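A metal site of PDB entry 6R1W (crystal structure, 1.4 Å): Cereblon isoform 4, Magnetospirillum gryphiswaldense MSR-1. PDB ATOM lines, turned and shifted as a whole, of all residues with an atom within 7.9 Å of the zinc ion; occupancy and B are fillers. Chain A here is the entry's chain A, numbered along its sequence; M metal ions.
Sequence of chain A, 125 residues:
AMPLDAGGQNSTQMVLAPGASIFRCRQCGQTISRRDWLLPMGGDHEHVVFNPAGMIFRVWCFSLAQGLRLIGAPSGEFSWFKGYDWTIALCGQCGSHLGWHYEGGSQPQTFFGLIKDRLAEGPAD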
ATOM      1  N   ARG A  24     -18.699  -6.206 -16.519  1.00  0.00           N
ATOM      2  CA  ARG A  24     -17.826  -7.341 -16.619  1.00  0.00           C
ATOM      3  C   ARG A  24     -18.262  -8.413 -15.661  1.00  0.00           C
ATOM      4  O   ARG A  24     -18.931  -8.132 -14.665  1.00  0.00           O
ATOM      5  CB  ARG A  24     -16.364  -6.869 -16.301  1.00  0.00           C
ATOM      6  CG  ARG A  24     -15.835  -5.963 -17.282  1.00  0.00           C
ATOM      7  CD  ARG A  24     -14.360  -5.573 -17.009  1.00  0.00           C
ATOM      8  NE  ARG A  24     -13.819  -4.746 -18.044  1.00  0.00           N
ATOM      9  CZ  ARG A  24     -13.560  -5.138 -19.245  1.00  0.00           C
ATOM     10  NH1 ARG A  24     -13.476  -6.429 -19.595  1.00  0.00           N
ATOM     11  NH2 ARG A  24     -13.287  -4.265 -20.206  1.00  0.00           N
ATOM     12  N   CYS A  25     -17.836  -9.654 -15.873  1.00  0.00           N
ATOM     13  CA  CYS A  25     -18.026 -10.720 -14.900  1.00  0.00           C
ATOM     14  C   CYS A  25     -17.354 -10.362 -13.617  1.00  0.00           C
ATOM     15  O   CYS A  25     -16.159 -10.032 -13.611  1.00  0.00           O
ATOM     16  CB  CYS A  25     -17.502 -12.021 -15.473  1.00  0.00           C
ATOM     17  SG  CYS A  25     -17.602 -13.372 -14.267  1.00  0.00           S
ATOM     18  N   ARG A  26     -18.070 -10.413 -12.496  1.00  0.00           N
ATOM     19  CA  ARG A  26     -17.488 -10.080 -11.189  1.00  0.00           C
ATOM     20  C   ARG A  26     -16.379 -11.014 -10.809  1.00  0.00           C
ATOM     21  O   ARG A  26     -15.507 -10.607  -9.997  1.00  0.00           O
ATOM     22  CB  ARG A  26     -18.621 -10.094 -10.140  1.00  0.00           C
ATOM     23  CG  ARG A  26     -18.197  -9.849  -8.728  1.00  0.00           C
ATOM     24  CD  ARG A  26     -19.394  -9.781  -7.844  1.00  0.00           C
ATOM     25  NE  ARG A  26     -18.946  -9.693  -6.485  1.00  0.00           N
ATOM     26  CZ  ARG A  26     -19.757  -9.645  -5.443  1.00  0.00           C
ATOM     27  NH1 ARG A  26     -21.054  -9.573  -5.593  1.00  0.00           N
ATOM     28  NH2 ARG A  26     -19.210  -9.603  -4.244  1.00  0.00           N
ATOM     29  N   GLN A  27     -16.430 -12.245 -11.269  1.00  0.00           N
ATOM     30  CA  GLN A  27     -15.418 -13.247 -10.849  1.00  0.00           C
ATOM     31  C   GLN A  27     -14.170 -13.179 -11.644  1.00  0.00           C
ATOM     32  O   GLN A  27     -13.067 -13.473 -11.112  1.00  0.00           O
ATOM     33  CB  GLN A  27     -16.001 -14.624 -10.898  1.00  0.00           C
ATOM     34  CG  GLN A  27     -17.168 -14.743 -10.026  1.00  0.00           C
ATOM     35  CD  GLN A  27     -16.935 -14.381  -8.565  1.00  0.00           C
ATOM     36  OE1 GLN A  27     -15.934 -14.689  -7.993  1.00  0.00           O
ATOM     37  NE2 GLN A  27     -17.894 -13.662  -7.988  1.00  0.00           N
ATOM     38  N   CYS A  28     -14.137 -12.740 -12.872  1.00  0.00           N
ATOM     39  CA  CYS A  28     -12.942 -12.816 -13.715  1.00  0.00           C
ATOM     40  C   CYS A  28     -12.702 -11.674 -14.599  1.00  0.00           C
ATOM     41  O   CYS A  28     -11.614 -11.552 -15.222  1.00  0.00           O
ATOM     42  CB  CYS A  28     -13.027 -14.099 -14.515  1.00  0.00           C
ATOM     43  SG  CYS A  28     -14.196 -14.012 -15.950  1.00  0.00           S
ATOM     44  N   GLY A  29     -13.620 -10.727 -14.794  1.00  0.00           N
ATOM     45  CA  GLY A  29     -13.411  -9.618 -15.644  1.00  0.00           C
ATOM     46  C   GLY A  29     -13.751  -9.700 -17.101  1.00  0.00           C
ATOM     47  O   GLY A  29     -13.670  -8.691 -17.822  1.00  0.00           O
ATOM     48  N   GLN A  30     -14.298 -10.856 -17.543  1.00  0.00           N
ATOM     49  CA  GLN A  30     -14.731 -10.950 -18.950  1.00  0.00           C
ATOM     50  C   GLN A  30     -15.739  -9.841 -19.253  1.00  0.00           C
ATOM     51  O   GLN A  30     -16.632  -9.588 -18.478  1.00  0.00           O
ATOM     52  CB  GLN A  30     -15.339 -12.349 -19.176  1.00  0.00           C
ATOM     53  CG  GLN A  30     -15.988 -12.548 -20.520  1.00  0.00           C
ATOM     54  CD  GLN A  30     -15.050 -12.515 -21.742  1.00  0.00           C
ATOM     55  OE1 GLN A  30     -14.042 -13.272 -21.809  1.00  0.00           O
ATOM     56  NE2 GLN A  30     -15.445 -11.715 -22.774  1.00  0.00           N
ATOM     57  N   THR A  31     -15.592  -9.210 -20.410  1.00  0.00           N
ATOM     58  CA  THR A  31     -16.566  -8.215 -20.860  1.00  0.00           C
ATOM     59  C   THR A  31     -17.881  -8.908 -21.164  1.00  0.00           C
ATOM     60  O   THR A  31     -17.872  -9.865 -21.903  1.00  0.00           O
ATOM     61  CB  THR A  31     -16.071  -7.554 -22.147  1.00  0.00           C
ATOM     62  OG1 THR A  31     -14.646  -7.278 -22.063  1.00  0.00           O
ATOM     63  CG2 THR A  31     -16.824  -6.385 -22.320  1.00  0.00           C
ATOM     64  N   ILE A  32     -18.977  -8.334 -20.615  1.00  0.00           N
ATOM     65  CA  ILE A  32     -20.316  -8.965 -20.740  1.00  0.00           C
ATOM     66  C   ILE A  32     -21.304  -8.015 -21.389  1.00  0.00           C
ATOM     67  O   ILE A  32     -22.001  -8.410 -22.327  1.00  0.00           O
ATOM     68  CB  ILE A  32     -20.847  -9.495 -19.430  1.00  0.00           C
ATOM     69  CG1 ILE A  32     -19.914 -10.495 -18.761  1.00  0.00           C
ATOM     70  CG2 ILE A  32     -22.237 -10.102 -19.669  1.00  0.00           C
ATOM     71  CD1 ILE A  32     -19.694 -11.753 -19.526  1.00  0.00           C
ATOM     72  N   GLY A  67     -19.518 -12.423 -24.465  1.00  0.00           N
ATOM     73  CA  GLY A  67     -18.612 -13.092 -23.481  1.00  0.00           C
ATOM     74  C   GLY A  67     -19.271 -14.157 -22.696  1.00  0.00           C
ATOM     75  O   GLY A  67     -18.656 -14.637 -21.730  1.00  0.00           O
ATOM     76  N   LEU A  90     -23.706 -18.727 -18.968  1.00  0.00           N
ATOM     77  CA  LEU A  90     -22.518 -18.727 -18.128  1.00  0.00           C
ATOM     78  C   LEU A  90     -21.550 -17.714 -18.638  1.00  0.00           C
ATOM     79  O   LEU A  90     -21.497 -17.460 -19.843  1.00  0.00           O
ATOM     80  CB  LEU A  90     -21.854 -20.083 -18.103  1.00  0.00           C
ATOM     81  CG  LEU A  90     -22.740 -21.293 -17.690  1.00  0.00           C
ATOM     82  CD1 LEU A  90     -21.899 -22.574 -17.681  1.00  0.00           C
ATOM     83  CD2 LEU A  90     -23.416 -21.049 -16.374  1.00  0.00           C
ATOM     84  N   CYS A  91     -20.730 -17.167 -17.765  1.00  0.00           N
ATOM     85  CA  CYS A  91     -19.508 -16.476 -18.239  1.00  0.00           C
ATOM     86  C   CYS A  91     -18.713 -17.421 -19.087  1.00  0.00           C
ATOM     87  O   CYS A  91     -18.363 -18.531 -18.688  1.00  0.00           O
ATOM     88  CB  CYS A  91     -18.690 -16.046 -17.054  1.00  0.00           C
ATOM     89  SG  CYS A  91     -17.145 -15.200 -17.542  1.00  0.00           S
ATOM     90  N   GLY A  92     -18.404 -16.973 -20.336  1.00  0.00           N
ATOM     91  CA  GLY A  92     -17.654 -17.830 -21.208  1.00  0.00           C
ATOM     92  C   GLY A  92     -16.246 -18.017 -20.858  1.00  0.00           C
ATOM     93  O   GLY A  92     -15.597 -18.935 -21.428  1.00  0.00           O
ATOM     94  N   GLN A  93     -15.714 -17.236 -19.944  1.00  0.00           N
ATOM     95  CA  GLN A  93     -14.352 -17.354 -19.528  1.00  0.00           C
ATOM     96  C   GLN A  93     -14.271 -18.244 -18.274  1.00  0.00           C
ATOM     97  O   GLN A  93     -13.609 -19.305 -18.307  1.00  0.00           O
ATOM     98  CB  GLN A  93     -13.773 -15.968 -19.303  1.00  0.00           C
ATOM     99  CG  GLN A  93     -12.345 -15.891 -18.853  1.00  0.00           C
ATOM    100  CD  GLN A  93     -11.705 -14.542 -19.104  1.00  0.00           C
ATOM    101  OE1 GLN A  93     -11.080 -14.341 -20.144  1.00  0.00           O
ATOM    102  NE2 GLN A  93     -11.918 -13.596 -18.234  1.00  0.00           N
ATOM    103  N   CYS A  94     -14.993 -17.869 -17.214  1.00  0.00           N
ATOM    104  CA  CYS A  94     -14.827 -18.598 -15.941  1.00  0.00           C
ATOM    105  C   CYS A  94     -15.952 -19.559 -15.596  1.00  0.00           C
ATOM    106  O   CYS A  94     -15.784 -20.315 -14.614  1.00  0.00           O
ATOM    107  CB  CYS A  94     -14.617 -17.667 -14.797  1.00  0.00           C
ATOM    108  SG  CYS A  94     -16.110 -16.830 -14.181  1.00  0.00           S
ATOM    109  N   GLY A  95     -17.089 -19.531 -16.280  1.00  0.00           N
ATOM    110  CA  GLY A  95     -18.189 -20.419 -15.974  1.00  0.00           C
ATOM    111  C   GLY A  95     -19.140 -19.944 -14.932  1.00  0.00           C
ATOM    112  O   GLY A  95     -20.137 -20.656 -14.691  1.00  0.00           O
ATOM    113  N   SER A  96     -18.957 -18.806 -14.331  1.00  0.00           N
ATOM    114  CA  SER A  96     -19.901 -18.243 -13.363  1.00  0.00           C
ATOM    115  C   SER A  96     -21.275 -18.116 -14.022  1.00  0.00           C
ATOM    116  O   SER A  96     -21.397 -17.718 -15.170  1.00  0.00           O
ATOM    117  CB  SER A  96     -19.433 -16.848 -12.958  1.00  0.00           C
ATOM    118  OG  SER A  96     -20.354 -16.191 -12.044  1.00  0.00           O
ATOM    119  N   HIS A  97     -22.325 -18.478 -13.292  1.00  0.00           N
ATOM    120  CA  HIS A  97     -23.671 -18.361 -13.850  1.00  0.00           C
ATOM    121  C   HIS A  97     -24.113 -16.926 -13.787  1.00  0.00           C
ATOM    122  O   HIS A  97     -24.400 -16.381 -12.706  1.00  0.00           O
ATOM    123  CB  HIS A  97     -24.630 -19.240 -13.094  1.00  0.00           C
ATOM    124  CG  HIS A  97     -26.011 -19.074 -13.553  1.00  0.00           C
ATOM    125  ND1 HIS A  97     -27.065 -19.349 -12.713  1.00  0.00           N
ATOM    126  CD2 HIS A  97     -26.521 -18.721 -14.765  1.00  0.00           C
ATOM    127  CE1 HIS A  97     -28.171 -19.118 -13.420  1.00  0.00           C
ATOM    128  NE2 HIS A  97     -27.894 -18.772 -14.672  1.00  0.00           N
ATOM    129  N   LEU A  98     -24.155 -16.234 -14.928  1.00  0.00           N
ATOM    130  CA  LEU A  98     -24.452 -14.843 -14.998  1.00  0.00           C
ATOM    131  C   LEU A  98     -25.884 -14.486 -15.290  1.00  0.00           C
ATOM    132  O   LEU A  98     -26.342 -13.387 -14.977  1.00  0.00           O
ATOM    133  CB  LEU A  98     -23.557 -14.100 -15.982  1.00  0.00           C
ATOM    134  CG  LEU A  98     -22.072 -14.116 -15.619  1.00  0.00           C
ATOM    135  CD1 LEU A  98     -21.259 -13.259 -16.548  1.00  0.00           C
ATOM    136  CD2 LEU A  98     -21.772 -13.729 -14.200  1.00  0.00           C
ATOM    137  N   ARG A 118     -23.827 -10.243  -9.912  1.00  0.00           N
ATOM    138  CA  ARG A 118     -22.771 -11.070 -10.446  1.00  0.00           C
ATOM    139  C   ARG A 118     -21.946 -10.377 -11.462  1.00  0.00           C
ATOM    140  O   ARG A 118     -21.045 -10.980 -12.115  1.00  0.00           O
ATOM    141  CB  ARG A 118     -23.391 -12.378 -10.927  1.00  0.00           C
ATOM    142  CG  ARG A 118     -24.091 -13.128  -9.766  1.00  0.00           C
ATOM    143  CD  ARG A 118     -24.524 -14.534 -10.169  1.00  0.00           C
ATOM    144  NE  ARG A 118     -25.296 -15.128  -9.100  1.00  0.00           N
ATOM    145  CZ  ARG A 118     -25.777 -16.375  -9.154  1.00  0.00           C
ATOM    146  NH1 ARG A 118     -25.455 -17.137 -10.151  1.00  0.00           N
ATOM    147  NH2 ARG A 118     -26.519 -16.852  -8.141  1.00  0.00           N
HETATM  148 ZN    ZN M   1     -16.257 -14.853 -15.372  1.00  0.00          ZN
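The zinc ion is bound by the side-chain sulfur (SG) of Cys 25, the side-chain sulfur (SG) of Cys 28, the side-chain sulfur (SG) of Cys 94 and the side-chain sulfur (SG) of Cys 91.
Four residues have an atom within 4 Å of the zinc ion: Cys 25, Cys 28, Cys 91 and Cys 94.
The side-chain sulfur of Cys 94 sits close to the backbone NH of Ser 96 (3.5 Å). N of Cys 25 lies within hydrogen-bond range of O of Gln 30. The backbone NH (N) of Gln 93 lies close to the side-chain sulfur (SG) of Cys 91, 3.5 Å away. The backbone NH of Cys 91 is in hydrogen-bond range of the backbone carbonyl oxygen of Ser 96, 2.7 Å away. N of Gln 27 sits close to SG of Cys 25 (3.4 Å). The side-chain sulfur (SG) of Cys 28 lies close to the side-chain amide nitrogen (NE2) of Gln 93 (3.3 Å). SG of Cys 28 sits close to N of Gln 30, 3.5 Å away.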
